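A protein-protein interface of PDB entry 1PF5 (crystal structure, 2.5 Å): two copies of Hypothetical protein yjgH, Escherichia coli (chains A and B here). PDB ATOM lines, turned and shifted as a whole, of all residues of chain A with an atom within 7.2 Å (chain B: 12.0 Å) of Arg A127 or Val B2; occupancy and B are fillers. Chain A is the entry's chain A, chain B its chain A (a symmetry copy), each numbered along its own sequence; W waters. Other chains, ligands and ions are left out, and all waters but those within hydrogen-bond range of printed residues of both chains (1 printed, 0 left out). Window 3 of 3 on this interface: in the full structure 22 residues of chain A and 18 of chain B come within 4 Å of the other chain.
NH2 of Arg A127 lies close to N of Val B2, 2.9 Å away. The backbone NH (N) of Glu B3 lies close to the guanidinium group (NH2) of Arg A127, at 3.2 Å.
The side-chain carboxylate of Asp A73 lies within salt-bridge range of the guanidinium group of Arg A127, 3.6 Å away. OE2 of Glu B3 sits at hydrogen-bond distance from N of Gly B28, at 3.3 Å. N of Phe B32 is in hydrogen-bond range of O of Ile B25 (2.8 Å). The backbone NH (N) of Ile A75 lies within hydrogen-bond range of the backbone carbonyl oxygen (O) of Ile A125, at 2.7 Å. N of Ile A125 sits at hydrogen-bond distance from O of Asp A76 (3.1 Å).
Among the printed residues, merely in contact across the chains: Ile A75 with Ile B25 (3.5 Å), Ile A75 with Ser B27 (3.6 Å), Ile A75 with Phe B32 (3.4 Å), Asp A76 with Phe B32 (3.6 Å), Ile A125 with Phe B32 (3.9 Å), Arg A127 with Arg B4 (3.8 Å) and Arg A127 with Ser B27 (3.8 Å).
Gly A28 touches none of the printed residues of chain B. No residue of chain B comes within 4 Å of Leu A30. No residue of chain B comes within 4 Å of Leu A31. No residue of chain B comes within 4 Å of Asp A72. No residue of chain B comes within 4 Å of Asp A73. Of the printed residues of chain B, Asp A76 touches Phe B32 (3.6 Å). Ala A126 touches none of the printed residues of chain B. No residue of chain B comes within 4 Å of Ile A128. No residue of chain B comes within 4 Å of Pro A129. Of the printed residues of chain A, Glu B3 touches Arg A127. Of the printed residues of chain A, Arg B4 touches Arg A127. Printed residues of chain A within 4 Å of Ile B25: Ile A75. Printed residues of chain A within 4 Å of Phe B32: Ile A75, Asp A76 and Ile A125. Glu B130 touches none of the printed residues of chain A. The nearest residue of chain B that does not touch Arg A127 is Gly B28 (6.9 Å). The nearest residue of chain A that does not touch Val B2 is Asp A72 (5.8 Å).
Of the 20 printed residues of chain A, 4 touch a printed residue of chain B. Among the printed residues, no Asp or Glu carboxylate lies within 4 Å of a Lys or Arg side-chain nitrogen of the other chain.
6 positions are printed for both chains. Of the 9 pairs that touch across the chains among the printed residues, none has its exchanged pair printed and touching as well.
Water W1 lies within hydrogen-bond range of OD2 of Asp A29 (2.9 Å) and OG of Ser B27 (3.4 Å).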
ATOM      1  N   ARG A  26       2.129 -34.971 -25.822  1.00  0.00           N
ATOM      2  CA  ARG A  26       2.279 -33.680 -25.168  1.00  0.00           C
ATOM      3  C   ARG A  26       3.744 -33.569 -24.774  1.00  0.00           C
ATOM      4  O   ARG A  26       4.273 -34.429 -24.073  1.00  0.00           O
ATOM      5  CB  ARG A  26       1.373 -33.598 -23.933  1.00  0.00           C
ATOM      6  CG  ARG A  26       1.653 -32.430 -22.978  1.00  0.00           C
ATOM      7  CD  ARG A  26       0.460 -32.223 -22.028  1.00  0.00           C
ATOM      8  NE  ARG A  26       0.740 -31.420 -20.830  1.00  0.00           N
ATOM      9  CZ  ARG A  26       1.321 -30.221 -20.824  1.00  0.00           C
ATOM     10  NH1 ARG A  26       1.711 -29.653 -21.960  1.00  0.00           N
ATOM     11  NH2 ARG A  26       1.493 -29.572 -19.675  1.00  0.00           N
ATOM     12  N   GLY A  28       6.218 -30.594 -23.331  1.00  0.00           N
ATOM     13  CA  GLY A  28       6.465 -29.233 -22.927  1.00  0.00           C
ATOM     14  C   GLY A  28       5.212 -28.428 -23.184  1.00  0.00           C
ATOM     15  O   GLY A  28       4.137 -28.768 -22.683  1.00  0.00           O
ATOM     16  N   ASP A  29       5.346 -27.377 -23.989  1.00  0.00           N
ATOM     17  CA  ASP A  29       4.228 -26.498 -24.304  1.00  0.00           C
ATOM     18  C   ASP A  29       3.598 -26.795 -25.662  1.00  0.00           C
ATOM     19  O   ASP A  29       2.887 -25.955 -26.223  1.00  0.00           O
ATOM     20  CB  ASP A  29       4.696 -25.038 -24.261  1.00  0.00           C
ATOM     21  CG  ASP A  29       5.819 -24.754 -25.249  1.00  0.00           C
ATOM     22  OD1 ASP A  29       6.882 -25.412 -25.154  1.00  0.00           O
ATOM     23  OD2 ASP A  29       5.638 -23.874 -26.124  1.00  0.00           O
ATOM     24  N   LEU A  30       3.854 -27.987 -26.193  1.00  0.00           N
ATOM     25  CA  LEU A  30       3.306 -28.356 -27.493  1.00  0.00           C
ATOM     26  C   LEU A  30       2.643 -29.720 -27.494  1.00  0.00           C
ATOM     27  O   LEU A  30       3.078 -30.645 -26.806  1.00  0.00           O
ATOM     28  CB  LEU A  30       4.406 -28.342 -28.557  1.00  0.00           C
ATOM     29  CG  LEU A  30       4.970 -27.004 -29.034  1.00  0.00           C
ATOM     30  CD1 LEU A  30       6.281 -27.264 -29.748  1.00  0.00           C
ATOM     31  CD2 LEU A  30       3.976 -26.299 -29.950  1.00  0.00           C
ATOM     32  N   LEU A  31       1.580 -29.829 -28.277  1.00  0.00           N
ATOM     33  CA  LEU A  31       0.853 -31.077 -28.415  1.00  0.00           C
ATOM     34  C   LEU A  31       0.929 -31.473 -29.882  1.00  0.00           C
ATOM     35  O   LEU A  31       0.443 -30.732 -30.744  1.00  0.00           O
ATOM     36  CB  LEU A  31      -0.613 -30.895 -28.030  1.00  0.00           C
ATOM     37  CG  LEU A  31      -1.398 -32.202 -28.042  1.00  0.00           C
ATOM     38  CD1 LEU A  31      -0.944 -33.067 -26.884  1.00  0.00           C
ATOM     39  CD2 LEU A  31      -2.880 -31.916 -27.945  1.00  0.00           C
ATOM     40  N   LEU A  64      -7.982 -33.649 -28.753  1.00  0.00           N
ATOM     41  CA  LEU A  64      -7.556 -32.370 -28.180  1.00  0.00           C
ATOM     42  C   LEU A  64      -8.087 -32.245 -26.742  1.00  0.00           C
ATOM     43  O   LEU A  64      -7.348 -31.894 -25.828  1.00  0.00           O
ATOM     44  CB  LEU A  64      -8.072 -31.203 -29.032  1.00  0.00           C
ATOM     45  CG  LEU A  64      -7.373 -30.919 -30.364  1.00  0.00           C
ATOM     46  CD1 LEU A  64      -8.126 -29.846 -31.125  1.00  0.00           C
ATOM     47  CD2 LEU A  64      -5.944 -30.471 -30.101  1.00  0.00           C
ATOM     48  N   GLY A  68      -6.817 -31.228 -22.745  1.00  0.00           N
ATOM     49  CA  GLY A  68      -7.337 -29.978 -22.232  1.00  0.00           C
ATOM     50  C   GLY A  68      -7.337 -28.912 -23.308  1.00  0.00           C
ATOM     51  O   GLY A  68      -7.489 -27.727 -23.010  1.00  0.00           O
ATOM     52  N   CYS A  69      -7.181 -29.332 -24.561  1.00  0.00           N
ATOM     53  CA  CYS A  69      -7.137 -28.404 -25.687  1.00  0.00           C
ATOM     54  C   CYS A  69      -8.446 -28.345 -26.445  1.00  0.00           C
ATOM     55  O   CYS A  69      -9.328 -29.182 -26.254  1.00  0.00           O
ATOM     56  CB  CYS A  69      -6.037 -28.801 -26.686  1.00  0.00           C
ATOM     57  SG  CYS A  69      -4.316 -28.910 -26.049  1.00  0.00           S
ATOM     58  N   THR A  70      -8.548 -27.347 -27.319  1.00  0.00           N
ATOM     59  CA  THR A  70      -9.719 -27.151 -28.166  1.00  0.00           C
ATOM     60  C   THR A  70      -9.180 -26.696 -29.516  1.00  0.00           C
ATOM     61  O   THR A  70      -7.974 -26.541 -29.669  1.00  0.00           O
ATOM     62  CB  THR A  70     -10.673 -26.061 -27.599  1.00  0.00           C
ATOM     63  OG1 THR A  70     -10.097 -24.761 -27.787  1.00  0.00           O
ATOM     64  CG2 THR A  70     -10.913 -26.288 -26.107  1.00  0.00           C
ATOM     65  N   ASP A  72      -9.200 -23.887 -30.734  1.00  0.00           N
ATOM     66  CA  ASP A  72      -8.597 -22.566 -30.611  1.00  0.00           C
ATOM     67  C   ASP A  72      -7.120 -22.616 -30.298  1.00  0.00           C
ATOM     68  O   ASP A  72      -6.414 -21.621 -30.461  1.00  0.00           O
ATOM     69  CB  ASP A  72      -9.303 -21.751 -29.528  1.00  0.00           C
ATOM     70  CG  ASP A  72     -10.757 -21.473 -29.861  1.00  0.00           C
ATOM     71  OD1 ASP A  72     -11.030 -20.997 -30.985  1.00  0.00           O
ATOM     72  OD2 ASP A  72     -11.626 -21.729 -28.996  1.00  0.00           O
ATOM     73  N   ASP A  73      -6.655 -23.773 -29.848  1.00  0.00           N
ATOM     74  CA  ASP A  73      -5.252 -23.943 -29.501  1.00  0.00           C
ATOM     75  C   ASP A  73      -4.406 -24.492 -30.644  1.00  0.00           C
ATOM     76  O   ASP A  73      -3.195 -24.655 -30.507  1.00  0.00           O
ATOM     77  CB  ASP A  73      -5.139 -24.852 -28.289  1.00  0.00           C
ATOM     78  CG  ASP A  73      -5.913 -24.318 -27.104  1.00  0.00           C
ATOM     79  OD1 ASP A  73      -5.582 -23.204 -26.633  1.00  0.00           O
ATOM     80  OD2 ASP A  73      -6.855 -25.007 -26.648  1.00  0.00           O
ATOM     81  N   ILE A  74      -5.045 -24.775 -31.772  1.00  0.00           N
ATOM     82  CA  ILE A  74      -4.335 -25.295 -32.930  1.00  0.00           C
ATOM     83  C   ILE A  74      -3.435 -24.207 -33.514  1.00  0.00           C
ATOM     84  O   ILE A  74      -3.903 -23.110 -33.828  1.00  0.00           O
ATOM     85  CB  ILE A  74      -5.337 -25.796 -34.001  1.00  0.00           C
ATOM     86  CG1 ILE A  74      -6.055 -27.042 -33.476  1.00  0.00           C
ATOM     87  CG2 ILE A  74      -4.619 -26.091 -35.316  1.00  0.00           C
ATOM     88  CD1 ILE A  74      -7.104 -27.572 -34.401  1.00  0.00           C
ATOM     89  N   ILE A  75      -2.146 -24.499 -33.656  1.00  0.00           N
ATOM     90  CA  ILE A  75      -1.232 -23.511 -34.208  1.00  0.00           C
ATOM     91  C   ILE A  75      -0.680 -23.881 -35.576  1.00  0.00           C
ATOM     92  O   ILE A  75      -0.037 -23.061 -36.235  1.00  0.00           O
ATOM     93  CB  ILE A  75      -0.080 -23.217 -33.243  1.00  0.00           C
ATOM     94  CG1 ILE A  75       0.654 -24.504 -32.881  1.00  0.00           C
ATOM     95  CG2 ILE A  75      -0.627 -22.547 -32.003  1.00  0.00           C
ATOM     96  CD1 ILE A  75       1.787 -24.289 -31.903  1.00  0.00           C
ATOM     97  N   ASP A  76      -0.933 -25.113 -36.004  1.00  0.00           N
ATOM     98  CA  ASP A  76      -0.494 -25.554 -37.323  1.00  0.00           C
ATOM     99  C   ASP A  76      -1.406 -26.659 -37.845  1.00  0.00           C
ATOM    100  O   ASP A  76      -1.753 -27.590 -37.117  1.00  0.00           O
ATOM    101  CB  ASP A  76       0.950 -26.039 -37.292  1.00  0.00           C
ATOM    102  CG  ASP A  76       1.473 -26.379 -38.680  1.00  0.00           C
ATOM    103  OD1 ASP A  76       1.844 -27.555 -38.896  1.00  0.00           O
ATOM    104  OD2 ASP A  76       1.507 -25.477 -39.555  1.00  0.00           O
ATOM    105  N   ILE A 125      -0.962 -29.407 -34.773  1.00  0.00           N
ATOM    106  CA  ILE A 125      -0.060 -29.128 -33.652  1.00  0.00           C
ATOM    107  C   ILE A 125      -0.761 -28.055 -32.826  1.00  0.00           C
ATOM    108  O   ILE A 125      -1.232 -27.056 -33.378  1.00  0.00           O
ATOM    109  CB  ILE A 125       1.312 -28.575 -34.089  1.00  0.00           C
ATOM    110  CG1 ILE A 125       2.015 -29.589 -34.990  1.00  0.00           C
ATOM    111  CG2 ILE A 125       2.171 -28.286 -32.854  1.00  0.00           C
ATOM    112  CD1 ILE A 125       3.403 -29.193 -35.389  1.00  0.00           C
ATOM    113  N   ALA A 126      -0.845 -28.262 -31.516  1.00  0.00           N
ATOM    114  CA  ALA A 126      -1.505 -27.299 -30.643  1.00  0.00           C
ATOM    115  C   ALA A 126      -0.583 -26.870 -29.508  1.00  0.00           C
ATOM    116  O   ALA A 126       0.293 -27.632 -29.091  1.00  0.00           O
ATOM    117  CB  ALA A 126      -2.779 -27.905 -30.081  1.00  0.00           C
ATOM    118  N   ARG A 127      -0.778 -25.650 -29.014  1.00  0.00           N
ATOM    119  CA  ARG A 127       0.046 -25.138 -27.921  1.00  0.00           C
ATOM    120  C   ARG A 127      -0.577 -25.460 -26.586  1.00  0.00           C
ATOM    121  O   ARG A 127      -1.750 -25.223 -26.380  1.00  0.00           O
ATOM    122  CB  ARG A 127       0.245 -23.621 -28.036  1.00  0.00           C
ATOM    123  CG  ARG A 127      -1.017 -22.846 -28.415  1.00  0.00           C
ATOM    124  CD  ARG A 127      -1.643 -22.042 -27.261  1.00  0.00           C
ATOM    125  NE  ARG A 127      -2.765 -21.223 -27.742  1.00  0.00           N
ATOM    126  CZ  ARG A 127      -3.450 -20.350 -26.998  1.00  0.00           C
ATOM    127  NH1 ARG A 127      -3.135 -20.163 -25.711  1.00  0.00           N
ATOM    128  NH2 ARG A 127      -4.453 -19.658 -27.545  1.00  0.00           N
ATOM    129  N   ILE A 128       0.226 -26.012 -25.689  1.00  0.00           N
ATOM    130  CA  ILE A 128      -0.233 -26.366 -24.365  1.00  0.00           C
ATOM    131  C   ILE A 128       0.609 -25.623 -23.350  1.00  0.00           C
ATOM    132  O   ILE A 128       1.667 -26.106 -22.956  1.00  0.00           O
ATOM    133  CB  ILE A 128      -0.062 -27.854 -24.095  1.00  0.00           C
ATOM    134  CG1 ILE A 128      -0.739 -28.665 -25.186  1.00  0.00           C
ATOM    135  CG2 ILE A 128      -0.685 -28.203 -22.770  1.00  0.00           C
ATOM    136  CD1 ILE A 128      -0.762 -30.150 -24.889  1.00  0.00           C
ATOM    137  N   PRO A 129       0.162 -24.434 -22.917  1.00  0.00           N
ATOM    138  CA  PRO A 129       0.934 -23.668 -21.933  1.00  0.00           C
ATOM    139  C   PRO A 129       1.261 -24.507 -20.693  1.00  0.00           C
ATOM    140  O   PRO A 129       0.373 -25.132 -20.110  1.00  0.00           O
ATOM    141  CB  PRO A 129       0.010 -22.495 -21.611  1.00  0.00           C
ATOM    142  CG  PRO A 129      -0.703 -22.271 -22.922  1.00  0.00           C
ATOM    143  CD  PRO A 129      -1.037 -23.687 -23.344  1.00  0.00           C
ATOM    144  N   GLU A 130       2.539 -24.528 -20.311  1.00  0.00           N
ATOM    145  CA  GLU A 130       2.987 -25.275 -19.134  1.00  0.00           C
ATOM    146  C   GLU A 130       2.954 -24.344 -17.916  1.00  0.00           C
ATOM    147  O   GLU A 130       3.896 -23.581 -17.669  1.00  0.00           O
ATOM    148  CB  GLU A 130       4.410 -25.827 -19.343  1.00  0.00           C
ATOM    149  CG  GLU A 130       5.042 -25.519 -20.704  1.00  0.00           C
ATOM    150  CD  GLU A 130       5.628 -24.110 -20.801  1.00  0.00           C
ATOM    151  OE1 GLU A 130       6.629 -23.836 -20.107  1.00  0.00           O
ATOM    152  OE2 GLU A 130       5.095 -23.278 -21.572  1.00  0.00           O
ATOM    153  N   VAL B   2      -5.599 -17.047 -27.068  1.00  0.00           N
ATOM    154  CA  VAL B   2      -4.778 -16.275 -26.081  1.00  0.00           C
ATOM    155  C   VAL B   2      -3.363 -16.050 -26.630  1.00  0.00           C
ATOM    156  O   VAL B   2      -2.630 -15.163 -26.165  1.00  0.00           O
ATOM    157  CB  VAL B   2      -4.677 -17.030 -24.721  1.00  0.00           C
ATOM    158  CG1 VAL B   2      -4.003 -16.143 -23.677  1.00  0.00           C
ATOM    159  CG2 VAL B   2      -6.066 -17.452 -24.248  1.00  0.00           C
ATOM    160  N   GLU B   3      -2.998 -16.860 -27.624  1.00  0.00           N
ATOM    161  CA  GLU B   3      -1.683 -16.792 -28.270  1.00  0.00           C
ATOM    162  C   GLU B   3      -1.827 -16.848 -29.805  1.00  0.00           C
ATOM    163  O   GLU B   3      -0.961 -16.348 -30.537  1.00  0.00           O
ATOM    164  CB  GLU B   3      -0.801 -17.958 -27.777  1.00  0.00           C
ATOM    165  CG  GLU B   3       0.625 -17.987 -28.337  1.00  0.00           C
ATOM    166  CD  GLU B   3       1.503 -16.858 -27.807  1.00  0.00           C
ATOM    167  OE1 GLU B   3       1.740 -16.818 -26.578  1.00  0.00           O
ATOM    168  OE2 GLU B   3       1.957 -16.016 -28.622  1.00  0.00           O
ATOM    169  N   ARG B   4      -2.930 -17.444 -30.275  1.00  0.00           N
ATOM    170  CA  ARG B   4      -3.216 -17.589 -31.706  1.00  0.00           C
ATOM    171  C   ARG B   4      -3.227 -16.255 -32.470  1.00  0.00           C
ATOM    172  O   ARG B   4      -4.296 -15.670 -32.709  1.00  0.00           O
ATOM    173  CB  ARG B   4      -4.557 -18.318 -31.896  1.00  0.00           C
ATOM    174  N   THR B   5      -2.035 -15.787 -32.856  1.00  0.00           N
ATOM    175  CA  THR B   5      -1.897 -14.532 -33.596  1.00  0.00           C
ATOM    176  C   THR B   5      -1.503 -14.780 -35.055  1.00  0.00           C
ATOM    177  O   THR B   5      -0.459 -15.363 -35.343  1.00  0.00           O
ATOM    178  CB  THR B   5      -0.854 -13.581 -32.930  1.00  0.00           C
ATOM    179  OG1 THR B   5       0.464 -14.104 -33.102  1.00  0.00           O
ATOM    180  CG2 THR B   5      -1.130 -13.444 -31.442  1.00  0.00           C
ATOM    181  N   ALA B   6      -2.358 -14.334 -35.970  1.00  0.00           N
ATOM    182  CA  ALA B   6      -2.135 -14.509 -37.399  1.00  0.00           C
ATOM    183  C   ALA B   6      -1.147 -13.505 -37.973  1.00  0.00           C
ATOM    184  O   ALA B   6      -1.070 -12.361 -37.529  1.00  0.00           O
ATOM    185  CB  ALA B   6      -3.461 -14.412 -38.151  1.00  0.00           C
ATOM    186  N   ILE B  25       1.278 -18.470 -38.353  1.00  0.00           N
ATOM    187  CA  ILE B  25       0.792 -18.344 -36.987  1.00  0.00           C
ATOM    188  C   ILE B  25       1.995 -18.246 -36.087  1.00  0.00           C
ATOM    189  O   ILE B  25       2.867 -19.111 -36.117  1.00  0.00           O
ATOM    190  CB  ILE B  25      -0.044 -19.569 -36.537  1.00  0.00           C
ATOM    191  CG1 ILE B  25      -1.359 -19.620 -37.312  1.00  0.00           C
ATOM    192  CG2 ILE B  25      -0.327 -19.494 -35.040  1.00  0.00           C
ATOM    193  CD1 ILE B  25      -2.223 -18.398 -37.131  1.00  0.00           C
ATOM    194  N   ARG B  26       2.051 -17.175 -35.306  1.00  0.00           N
ATOM    195  CA  ARG B  26       3.142 -16.975 -34.365  1.00  0.00           C
ATOM    196  C   ARG B  26       2.648 -17.489 -33.021  1.00  0.00           C
ATOM    197  O   ARG B  26       1.613 -17.050 -32.524  1.00  0.00           O
ATOM    198  CB  ARG B  26       3.509 -15.488 -34.281  1.00  0.00           C
ATOM    199  CG  ARG B  26       4.421 -15.091 -33.111  1.00  0.00           C
ATOM    200  CD  ARG B  26       5.029 -13.701 -33.360  1.00  0.00           C
ATOM    201  NE  ARG B  26       5.593 -13.038 -32.175  1.00  0.00           N
ATOM    202  CZ  ARG B  26       6.465 -13.584 -31.329  1.00  0.00           C
ATOM    203  NH1 ARG B  26       6.893 -14.829 -31.509  1.00  0.00           N
ATOM    204  NH2 ARG B  26       6.932 -12.872 -30.307  1.00  0.00           N
ATOM    205  N   SER B  27       3.368 -18.442 -32.449  1.00  0.00           N
ATOM    206  CA  SER B  27       2.972 -19.001 -31.172  1.00  0.00           C
ATOM    207  C   SER B  27       4.183 -19.175 -30.277  1.00  0.00           C
ATOM    208  O   SER B  27       4.963 -20.121 -30.430  1.00  0.00           O
ATOM    209  CB  SER B  27       2.283 -20.345 -31.370  1.00  0.00           C
ATOM    210  OG  SER B  27       1.925 -20.909 -30.123  1.00  0.00           O
ATOM    211  N   GLY B  28       4.330 -18.258 -29.330  1.00  0.00           N
ATOM    212  CA  GLY B  28       5.461 -18.327 -28.439  1.00  0.00           C
ATOM    213  C   GLY B  28       6.706 -17.994 -29.229  1.00  0.00           C
ATOM    214  O   GLY B  28       6.790 -16.927 -29.843  1.00  0.00           O
ATOM    215  N   ASP B  29       7.661 -18.921 -29.234  1.00  0.00           N
ATOM    216  CA  ASP B  29       8.924 -18.724 -29.933  1.00  0.00           C
ATOM    217  C   ASP B  29       8.971 -19.419 -31.290  1.00  0.00           C
ATOM    218  O   ASP B  29      10.051 -19.640 -31.847  1.00  0.00           O
ATOM    219  CB  ASP B  29      10.078 -19.227 -29.056  1.00  0.00           C
ATOM    220  CG  ASP B  29       9.949 -20.704 -28.710  1.00  0.00           C
ATOM    221  OD1 ASP B  29       8.922 -21.091 -28.104  1.00  0.00           O
ATOM    222  OD2 ASP B  29      10.874 -21.480 -29.047  1.00  0.00           O
ATOM    223  N   LEU B  30       7.804 -19.763 -31.828  1.00  0.00           N
ATOM    224  CA  LEU B  30       7.750 -20.443 -33.116  1.00  0.00           C
ATOM    225  C   LEU B  30       6.758 -19.816 -34.078  1.00  0.00           C
ATOM    226  O   LEU B  30       5.701 -19.323 -33.679  1.00  0.00           O
ATOM    227  CB  LEU B  30       7.386 -21.917 -32.926  1.00  0.00           C
ATOM    228  CG  LEU B  30       8.418 -22.871 -32.325  1.00  0.00           C
ATOM    229  CD1 LEU B  30       7.702 -24.127 -31.871  1.00  0.00           C
ATOM    230  CD2 LEU B  30       9.505 -23.197 -33.343  1.00  0.00           C
ATOM    231  N   LEU B  31       7.117 -19.840 -35.354  1.00  0.00           N
ATOM    232  CA  LEU B  31       6.265 -19.311 -36.401  1.00  0.00           C
ATOM    233  C   LEU B  31       5.949 -20.467 -37.339  1.00  0.00           C
ATOM    234  O   LEU B  31       6.867 -21.037 -37.941  1.00  0.00           O
ATOM    235  CB  LEU B  31       6.988 -18.222 -37.188  1.00  0.00           C
ATOM    236  CG  LEU B  31       6.098 -17.547 -38.226  1.00  0.00           C
ATOM    237  CD1 LEU B  31       5.063 -16.696 -37.518  1.00  0.00           C
ATOM    238  CD2 LEU B  31       6.938 -16.702 -39.157  1.00  0.00           C
ATOM    239  N   PHE B  32       4.672 -20.837 -37.444  1.00  0.00           N
ATOM    240  CA  PHE B  32       4.270 -21.913 -38.348  1.00  0.00           C
ATOM    241  C   PHE B  32       3.656 -21.275 -39.584  1.00  0.00           C
ATOM    242  O   PHE B  32       2.568 -20.705 -39.520  1.00  0.00           O
ATOM    243  CB  PHE B  32       3.254 -22.842 -37.691  1.00  0.00           C
ATOM    244  CG  PHE B  32       3.792 -23.580 -36.514  1.00  0.00           C
ATOM    245  CD1 PHE B  32       3.800 -22.991 -35.251  1.00  0.00           C
ATOM    246  CD2 PHE B  32       4.314 -24.863 -36.664  1.00  0.00           C
ATOM    247  CE1 PHE B  32       4.327 -23.674 -34.148  1.00  0.00           C
ATOM    248  CE2 PHE B  32       4.841 -25.551 -35.574  1.00  0.00           C
ATOM    249  CZ  PHE B  32       4.848 -24.956 -34.312  1.00  0.00           C
ATOM    250  N   GLU B 130      11.184 -14.928 -28.156  1.00  0.00           N
ATOM    251  CA  GLU B 130      10.260 -14.081 -27.399  1.00  0.00           C
ATOM    252  C   GLU B 130      11.063 -13.253 -26.388  1.00  0.00           C
ATOM    253  O   GLU B 130      11.381 -13.720 -25.289  1.00  0.00           O
ATOM    254  CB  GLU B 130       9.205 -14.933 -26.669  1.00  0.00           C
ATOM    255  CG  GLU B 130       9.312 -16.445 -26.894  1.00  0.00           C
ATOM    256  CD  GLU B 130      10.380 -17.117 -26.030  1.00  0.00           C
ATOM    257  OE1 GLU B 130      10.201 -17.162 -24.794  1.00  0.00           O
ATOM    258  OE2 GLU B 130      11.394 -17.605 -26.582  1.00  0.00           O
HETATM  259  O   HOH W   1       3.807 -22.991 -28.223  1.00  0.00           O
